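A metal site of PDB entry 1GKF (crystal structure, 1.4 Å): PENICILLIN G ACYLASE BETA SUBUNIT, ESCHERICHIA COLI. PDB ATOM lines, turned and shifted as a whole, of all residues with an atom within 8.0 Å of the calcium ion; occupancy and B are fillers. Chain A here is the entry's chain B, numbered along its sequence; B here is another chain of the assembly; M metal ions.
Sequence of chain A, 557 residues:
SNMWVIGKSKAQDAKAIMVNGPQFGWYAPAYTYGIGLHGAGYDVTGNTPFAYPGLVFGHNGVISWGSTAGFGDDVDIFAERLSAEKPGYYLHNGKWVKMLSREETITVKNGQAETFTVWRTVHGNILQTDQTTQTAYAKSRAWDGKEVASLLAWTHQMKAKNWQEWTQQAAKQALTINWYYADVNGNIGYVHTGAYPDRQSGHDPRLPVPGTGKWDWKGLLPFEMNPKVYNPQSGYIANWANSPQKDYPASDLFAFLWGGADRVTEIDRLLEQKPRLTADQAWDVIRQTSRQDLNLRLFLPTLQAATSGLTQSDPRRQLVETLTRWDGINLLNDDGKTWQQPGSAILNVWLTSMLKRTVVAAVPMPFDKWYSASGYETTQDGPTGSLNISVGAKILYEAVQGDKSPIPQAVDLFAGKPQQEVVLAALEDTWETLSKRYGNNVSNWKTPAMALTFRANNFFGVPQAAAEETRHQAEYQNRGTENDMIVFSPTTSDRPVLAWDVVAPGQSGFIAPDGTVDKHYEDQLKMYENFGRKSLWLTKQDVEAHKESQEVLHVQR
The side-chain hydroxyl (OG1) of Thr 150 of chain B sits close to the backbone NH (N) of Glu 152 of chain B (3.4 Å).
The side-chain carboxylate of Glu 152 of chain B sits at hydrogen-bond distance from the backbone NH of Ile 77, 2.7 Å away.
The side-chain carboxylate (OD1) of Asp 252 is in hydrogen-bond range of the backbone NH (N) of Ser 151 of chain B, 2.8 Å away.
The side-chain amide nitrogen of Asn 155 of chain B lies within hydrogen-bond range of the backbone carbonyl oxygen of Asp 252.
OD2 of Asp 76 lies within salt-bridge range of NE of Arg 199 (2.8 Å).
The side-chain carboxylate (OD2) of Asp 76 sits close to a ring nitrogen (NE2) of His 203, 3.3 Å away.
The indole nitrogen (NE1) of Trp 217 sits at hydrogen-bond distance from the side-chain carboxylate (OD2) of Asp 76 (2.9 Å).
N of Ser 140 is in hydrogen-bond range of O of Asp 76.
The nearest printed residue that does not touch the calcium ion is Arg 199 (4.1 Å).
OE2 of Glu 152 of chain B is bound to the calcium ion, 2.4 Å away.
The calcium ion is bound by OD2 of Asp 252, 2.4 Å away.
The calcium ion is bound by OD1 of Asp 76 (2.5 Å).
The calcium ion is bound by O of Val 75, 2.5 Å away.
The backbone carbonyl oxygen (O) of Pro 205 is bound to the calcium ion, 2.5 Å away.
The calcium ion is bound by the side-chain carboxylate (OD2) of Asp 73.
OD1 of Asp 73 binds the calcium ion, 2.6 Å away.
The calcium ion has seven donor atoms within binding distance.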
ATOM      1  N   GLY A  72     -17.170  12.219   8.650  1.00  0.00           N
ATOM      2  CA  GLY A  72     -16.578  13.527   8.362  1.00  0.00           C
ATOM      3  C   GLY A  72     -17.636  14.391   7.680  1.00  0.00           C
ATOM      4  O   GLY A  72     -18.673  13.933   7.278  1.00  0.00           O
ATOM      5  N   ASP A  73     -17.307  15.681   7.564  1.00  0.00           N
ATOM      6  CA  ASP A  73     -18.242  16.612   6.905  1.00  0.00           C
ATOM      7  C   ASP A  73     -17.887  16.734   5.440  1.00  0.00           C
ATOM      8  O   ASP A  73     -17.028  17.526   5.003  1.00  0.00           O
ATOM      9  CB  ASP A  73     -18.206  17.973   7.606  1.00  0.00           C
ATOM     10  CG  ASP A  73     -19.243  18.869   7.001  1.00  0.00           C
ATOM     11  OD1 ASP A  73     -19.877  18.538   5.955  1.00  0.00           O
ATOM     12  OD2 ASP A  73     -19.484  19.990   7.554  1.00  0.00           O
ATOM     13  N   ASP A  74     -18.529  15.889   4.647  1.00  0.00           N
ATOM     14  CA  ASP A  74     -18.310  15.833   3.202  1.00  0.00           C
ATOM     15  C   ASP A  74     -19.503  16.349   2.440  1.00  0.00           C
ATOM     16  O   ASP A  74     -19.631  16.068   1.209  1.00  0.00           O
ATOM     17  CB  ASP A  74     -17.919  14.424   2.753  1.00  0.00           C
ATOM     18  CG  ASP A  74     -18.928  13.357   3.047  1.00  0.00           C
ATOM     19  OD1 ASP A  74     -19.953  13.631   3.685  1.00  0.00           O
ATOM     20  OD2 ASP A  74     -18.719  12.174   2.639  1.00  0.00           O
ATOM     21  N   VAL A  75     -20.466  17.018   3.078  1.00  0.00           N
ATOM     22  CA  VAL A  75     -21.709  17.517   2.478  1.00  0.00           C
ATOM     23  C   VAL A  75     -21.976  18.924   2.899  1.00  0.00           C
ATOM     24  O   VAL A  75     -22.067  19.161   4.112  1.00  0.00           O
ATOM     25  CB  VAL A  75     -22.920  16.626   2.835  1.00  0.00           C
ATOM     26  CG1 VAL A  75     -24.170  17.190   2.190  1.00  0.00           C
ATOM     27  CG2 VAL A  75     -22.712  15.182   2.407  1.00  0.00           C
ATOM     28  N   ASP A  76     -22.130  19.858   1.968  1.00  0.00           N
ATOM     29  CA  ASP A  76     -22.496  21.221   2.280  1.00  0.00           C
ATOM     30  C   ASP A  76     -23.716  21.598   1.449  1.00  0.00           C
ATOM     31  O   ASP A  76     -23.923  20.999   0.373  1.00  0.00           O
ATOM     32  CB  ASP A  76     -21.397  22.239   2.027  1.00  0.00           C
ATOM     33  CG  ASP A  76     -20.155  22.083   2.785  1.00  0.00           C
ATOM     34  OD1 ASP A  76     -20.140  21.491   3.896  1.00  0.00           O
ATOM     35  OD2 ASP A  76     -19.054  22.546   2.396  1.00  0.00           O
ATOM     36  N   ILE A  77     -24.521  22.524   1.936  1.00  0.00           N
ATOM     37  CA  ILE A  77     -25.731  22.968   1.238  1.00  0.00           C
ATOM     38  C   ILE A  77     -25.505  24.374   0.694  1.00  0.00           C
ATOM     39  O   ILE A  77     -25.167  25.332   1.420  1.00  0.00           O
ATOM     40  CB  ILE A  77     -26.910  22.999   2.263  1.00  0.00           C
ATOM     41  CG1 ILE A  77     -27.347  21.558   2.571  1.00  0.00           C
ATOM     42  CG2 ILE A  77     -28.044  23.881   1.741  1.00  0.00           C
ATOM     43  CD1 ILE A  77     -28.422  21.296   3.588  1.00  0.00           C
ATOM     44  N   SER A 140     -24.535  19.543  -1.915  1.00  0.00           N
ATOM     45  CA  SER A 140     -23.236  19.244  -2.512  1.00  0.00           C
ATOM     46  C   SER A 140     -22.393  18.207  -1.779  1.00  0.00           C
ATOM     47  O   SER A 140     -21.898  18.450  -0.673  1.00  0.00           O
ATOM     48  CB  SER A 140     -22.411  20.557  -2.484  1.00  0.00           C
ATOM     49  OG  SER A 140     -21.261  20.409  -3.319  1.00  0.00           O
ATOM     50  N   PRO A 197     -14.055  18.559   0.712  1.00  0.00           N
ATOM     51  CA  PRO A 197     -13.907  19.785  -0.105  1.00  0.00           C
ATOM     52  C   PRO A 197     -12.815  20.689   0.427  1.00  0.00           C
ATOM     53  O   PRO A 197     -12.639  20.839   1.645  1.00  0.00           O
ATOM     54  CB  PRO A 197     -15.311  20.454   0.020  1.00  0.00           C
ATOM     55  CG  PRO A 197     -15.794  19.996   1.402  1.00  0.00           C
ATOM     56  CD  PRO A 197     -15.260  18.575   1.554  1.00  0.00           C
ATOM     57  N   ARG A 199     -12.484  24.231   0.984  1.00  0.00           N
ATOM     58  CA  ARG A 199     -13.433  25.316   1.144  1.00  0.00           C
ATOM     59  C   ARG A 199     -12.746  26.687   1.107  1.00  0.00           C
ATOM     60  O   ARG A 199     -11.616  26.835   1.540  1.00  0.00           O
ATOM     61  CB  ARG A 199     -14.197  25.113   2.488  1.00  0.00           C
ATOM     62  CG  ARG A 199     -15.016  23.799   2.500  1.00  0.00           C
ATOM     63  CD  ARG A 199     -15.755  23.679   3.808  1.00  0.00           C
ATOM     64  NE  ARG A 199     -16.717  22.548   3.892  1.00  0.00           N
ATOM     65  CZ  ARG A 199     -16.420  21.397   4.505  1.00  0.00           C
ATOM     66  NH1 ARG A 199     -15.266  21.087   5.014  1.00  0.00           N
ATOM     67  NH2 ARG A 199     -17.427  20.519   4.519  1.00  0.00           N
ATOM     68  N   HIS A 203     -15.548  29.983   5.140  1.00  0.00           N
ATOM     69  CA  HIS A 203     -16.702  29.079   5.054  1.00  0.00           C
ATOM     70  C   HIS A 203     -16.834  28.190   6.335  1.00  0.00           C
ATOM     71  O   HIS A 203     -15.968  27.373   6.595  1.00  0.00           O
ATOM     72  CB  HIS A 203     -16.482  28.201   3.829  1.00  0.00           C
ATOM     73  CG  HIS A 203     -17.517  27.173   3.495  1.00  0.00           C
ATOM     74  ND1 HIS A 203     -17.524  26.593   2.262  1.00  0.00           N
ATOM     75  CD2 HIS A 203     -18.529  26.645   4.262  1.00  0.00           C
ATOM     76  CE1 HIS A 203     -18.535  25.683   2.269  1.00  0.00           C
ATOM     77  NE2 HIS A 203     -19.141  25.715   3.472  1.00  0.00           N
ATOM     78  N   ASP A 204     -17.922  28.512   7.051  1.00  0.00           N
ATOM     79  CA  ASP A 204     -18.237  27.688   8.273  1.00  0.00           C
ATOM     80  C   ASP A 204     -19.034  26.494   7.754  1.00  0.00           C
ATOM     81  O   ASP A 204     -20.141  26.618   7.267  1.00  0.00           O
ATOM     82  CB  ASP A 204     -19.086  28.559   9.180  1.00  0.00           C
ATOM     83  CG  ASP A 204     -19.493  27.910  10.486  1.00  0.00           C
ATOM     84  OD1 ASP A 204     -19.576  26.655  10.566  1.00  0.00           O
ATOM     85  OD2 ASP A 204     -19.745  28.641  11.461  1.00  0.00           O
ATOM     86  N   PRO A 205     -18.451  25.301   7.854  1.00  0.00           N
ATOM     87  CA  PRO A 205     -19.029  24.106   7.235  1.00  0.00           C
ATOM     88  C   PRO A 205     -20.264  23.580   7.930  1.00  0.00           C
ATOM     89  O   PRO A 205     -20.865  22.622   7.418  1.00  0.00           O
ATOM     90  CB  PRO A 205     -17.914  23.057   7.255  1.00  0.00           C
ATOM     91  CG  PRO A 205     -17.153  23.454   8.494  1.00  0.00           C
ATOM     92  CD  PRO A 205     -17.157  24.992   8.479  1.00  0.00           C
ATOM     93  N   ARG A 206     -20.737  24.153   9.012  1.00  0.00           N
ATOM     94  CA  ARG A 206     -21.967  23.714   9.680  1.00  0.00           C
ATOM     95  C   ARG A 206     -23.191  24.373   9.118  1.00  0.00           C
ATOM     96  O   ARG A 206     -24.312  24.016   9.544  1.00  0.00           O
ATOM     97  CB  ARG A 206     -21.864  24.062  11.177  1.00  0.00           C
ATOM     98  CG  ARG A 206     -20.689  23.411  11.844  1.00  0.00           C
ATOM     99  CD  ARG A 206     -20.445  24.028  13.239  1.00  0.00           C
ATOM    100  NE  ARG A 206     -20.060  25.450  13.116  1.00  0.00           N
ATOM    101  CZ  ARG A 206     -19.912  26.212  14.154  1.00  0.00           C
ATOM    102  NH1 ARG A 206     -19.950  25.771  15.420  1.00  0.00           N
ATOM    103  NH2 ARG A 206     -19.596  27.511  14.010  1.00  0.00           N
ATOM    104  N   LEU A 207     -23.057  25.380   8.230  1.00  0.00           N
ATOM    105  CA  LEU A 207     -24.164  26.190   7.797  1.00  0.00           C
ATOM    106  C   LEU A 207     -24.125  26.430   6.292  1.00  0.00           C
ATOM    107  O   LEU A 207     -23.042  26.358   5.708  1.00  0.00           O
ATOM    108  CB  LEU A 207     -24.063  27.534   8.559  1.00  0.00           C
ATOM    109  CG  LEU A 207     -24.202  27.442  10.076  1.00  0.00           C
ATOM    110  CD1 LEU A 207     -23.588  28.652  10.766  1.00  0.00           C
ATOM    111  CD2 LEU A 207     -25.655  27.292  10.464  1.00  0.00           C
ATOM    112  N   PRO A 208     -25.234  26.731   5.668  1.00  0.00           N
ATOM    113  CA  PRO A 208     -25.299  26.831   4.211  1.00  0.00           C
ATOM    114  C   PRO A 208     -24.427  27.949   3.657  1.00  0.00           C
ATOM    115  O   PRO A 208     -24.134  28.904   4.380  1.00  0.00           O
ATOM    116  CB  PRO A 208     -26.767  27.044   3.876  1.00  0.00           C
ATOM    117  CG  PRO A 208     -27.516  26.489   5.089  1.00  0.00           C
ATOM    118  CD  PRO A 208     -26.597  26.855   6.245  1.00  0.00           C
ATOM    119  N   VAL A 209     -24.029  27.796   2.402  1.00  0.00           N
ATOM    120  CA  VAL A 209     -23.210  28.824   1.733  1.00  0.00           C
ATOM    121  C   VAL A 209     -23.983  29.361   0.553  1.00  0.00           C
ATOM    122  O   VAL A 209     -24.720  28.625  -0.109  1.00  0.00           O
ATOM    123  CB  VAL A 209     -21.879  28.258   1.190  1.00  0.00           C
ATOM    124  CG1 VAL A 209     -20.771  28.451   2.202  1.00  0.00           C
ATOM    125  CG2 VAL A 209     -21.937  26.746   0.884  1.00  0.00           C
ATOM    126  N   TRP A 217     -16.707  25.557  -3.698  1.00  0.00           N
ATOM    127  CA  TRP A 217     -15.508  24.879  -3.265  1.00  0.00           C
ATOM    128  C   TRP A 217     -14.348  25.144  -4.264  1.00  0.00           C
ATOM    129  O   TRP A 217     -14.652  25.207  -5.482  1.00  0.00           O
ATOM    130  CB  TRP A 217     -15.798  23.366  -3.230  1.00  0.00           C
ATOM    131  CG  TRP A 217     -16.770  22.911  -2.148  1.00  0.00           C
ATOM    132  CD1 TRP A 217     -17.131  23.543  -0.995  1.00  0.00           C
ATOM    133  CD2 TRP A 217     -17.468  21.656  -2.154  1.00  0.00           C
ATOM    134  NE1 TRP A 217     -17.987  22.752  -0.279  1.00  0.00           N
ATOM    135  CE2 TRP A 217     -18.219  21.583  -0.973  1.00  0.00           C
ATOM    136  CE3 TRP A 217     -17.481  20.601  -3.072  1.00  0.00           C
ATOM    137  CZ2 TRP A 217     -18.979  20.460  -0.615  1.00  0.00           C
ATOM    138  CZ3 TRP A 217     -18.285  19.509  -2.740  1.00  0.00           C
ATOM    139  CH2 TRP A 217     -19.003  19.444  -1.530  1.00  0.00           C
ATOM    140  N   ALA A 250     -16.111  16.976  12.796  1.00  0.00           N
ATOM    141  CA  ALA A 250     -17.189  16.064  12.561  1.00  0.00           C
ATOM    142  C   ALA A 250     -18.212  16.525  11.538  1.00  0.00           C
ATOM    143  O   ALA A 250     -18.282  17.712  11.199  1.00  0.00           O
ATOM    144  CB  ALA A 250     -17.992  15.903  13.874  1.00  0.00           C
ATOM    145  N   SER A 251     -19.021  15.573  11.099  1.00  0.00           N
ATOM    146  CA  SER A 251     -20.265  15.819  10.381  1.00  0.00           C
ATOM    147  C   SER A 251     -20.969  17.049  10.997  1.00  0.00           C
ATOM    148  O   SER A 251     -20.972  17.248  12.230  1.00  0.00           O
ATOM    149  CB  SER A 251     -21.158  14.578  10.679  1.00  0.00           C
ATOM    150  OG  SER A 251     -22.439  14.750  10.109  1.00  0.00           O
ATOM    151  N   ASP A 252     -21.686  17.778  10.130  1.00  0.00           N
ATOM    152  CA  ASP A 252     -22.457  18.915  10.594  1.00  0.00           C
ATOM    153  C   ASP A 252     -23.803  18.611  11.227  1.00  0.00           C
ATOM    154  O   ASP A 252     -24.444  19.512  11.735  1.00  0.00           O
ATOM    155  CB  ASP A 252     -22.611  19.959   9.454  1.00  0.00           C
ATOM    156  CG  ASP A 252     -23.461  19.442   8.342  1.00  0.00           C
ATOM    157  OD1 ASP A 252     -24.529  18.872   8.615  1.00  0.00           O
ATOM    158  OD2 ASP A 252     -23.100  19.619   7.152  1.00  0.00           O
ATOM    159  N   LEU A 253     -24.164  17.334  11.334  1.00  0.00           N
ATOM    160  CA  LEU A 253     -25.453  16.985  11.957  1.00  0.00           C
ATOM    161  C   LEU A 253     -25.539  17.531  13.402  1.00  0.00           C
ATOM    162  O   LEU A 253     -24.656  17.305  14.221  1.00  0.00           O
ATOM    163  CB  LEU A 253     -25.599  15.476  12.095  1.00  0.00           C
ATOM    164  CG  LEU A 253     -25.773  14.683  10.810  1.00  0.00           C
ATOM    165  CD1 LEU A 253     -25.788  13.203  11.229  1.00  0.00           C
ATOM    166  CD2 LEU A 253     -27.090  15.011  10.117  1.00  0.00           C
ATOM    167  N   SER B 149     -24.913  12.743   5.079  1.00  0.00           N
ATOM    168  CA  SER B 149     -25.494  13.316   6.281  1.00  0.00           C
ATOM    169  C   SER B 149     -25.232  14.785   6.442  1.00  0.00           C
ATOM    170  O   SER B 149     -24.075  15.216   6.571  1.00  0.00           O
ATOM    171  CB  SER B 149     -24.826  12.651   7.488  1.00  0.00           C
ATOM    172  OG  SER B 149     -25.235  11.303   7.639  1.00  0.00           O
ATOM    173  N   THR B 150     -26.289  15.590   6.422  1.00  0.00           N
ATOM    174  CA  THR B 150     -26.165  17.020   6.684  1.00  0.00           C
ATOM    175  C   THR B 150     -27.456  17.482   7.377  1.00  0.00           C
ATOM    176  O   THR B 150     -28.538  16.948   7.105  1.00  0.00           O
ATOM    177  CB  THR B 150     -25.833  17.832   5.412  1.00  0.00           C
ATOM    178  OG1 THR B 150     -25.543  19.188   5.794  1.00  0.00           O
ATOM    179  CG2 THR B 150     -26.995  17.852   4.412  1.00  0.00           C
ATOM    180  N   SER B 151     -27.292  18.525   8.213  1.00  0.00           N
ATOM    181  CA  SER B 151     -28.461  19.146   8.808  1.00  0.00           C
ATOM    182  C   SER B 151     -28.260  20.688   8.720  1.00  0.00           C
ATOM    183  O   SER B 151     -28.825  21.408   9.563  1.00  0.00           O
ATOM    184  CB  SER B 151     -28.786  18.721  10.242  1.00  0.00           C
ATOM    185  OG  SER B 151     -27.758  19.099  11.127  1.00  0.00           O
ATOM    186  N   GLU B 152     -27.553  21.208   7.678  1.00  0.00           N
ATOM    187  CA  GLU B 152     -27.212  22.628   7.691  1.00  0.00           C
ATOM    188  C   GLU B 152     -28.428  23.542   7.675  1.00  0.00           C
ATOM    189  O   GLU B 152     -28.324  24.623   8.318  1.00  0.00           O
ATOM    190  CB  GLU B 152     -26.338  23.013   6.457  1.00  0.00           C
ATOM    191  CG  GLU B 152     -24.937  22.368   6.558  1.00  0.00           C
ATOM    192  CD  GLU B 152     -24.100  22.769   5.382  1.00  0.00           C
ATOM    193  OE1 GLU B 152     -24.498  23.533   4.493  1.00  0.00           O
ATOM    194  OE2 GLU B 152     -22.924  22.322   5.294  1.00  0.00           O
ATOM    195  N   ASN B 155     -29.587  23.561  11.175  1.00  0.00           N
ATOM    196  CA  ASN B 155     -28.577  24.263  11.976  1.00  0.00           C
ATOM    197  C   ASN B 155     -28.798  25.754  11.868  1.00  0.00           C
ATOM    198  O   ASN B 155     -28.636  26.482  12.859  1.00  0.00           O
ATOM    199  CB  ASN B 155     -27.177  23.847  11.528  1.00  0.00           C
ATOM    200  CG  ASN B 155     -26.853  22.390  11.745  1.00  0.00           C
ATOM    201  OD1 ASN B 155     -27.598  21.610  12.329  1.00  0.00           O
ATOM    202  ND2 ASN B 155     -25.681  22.018  11.192  1.00  0.00           N
HETATM  203 CA    CA M   1     -21.315  20.686   5.897  1.00  0.00          CA
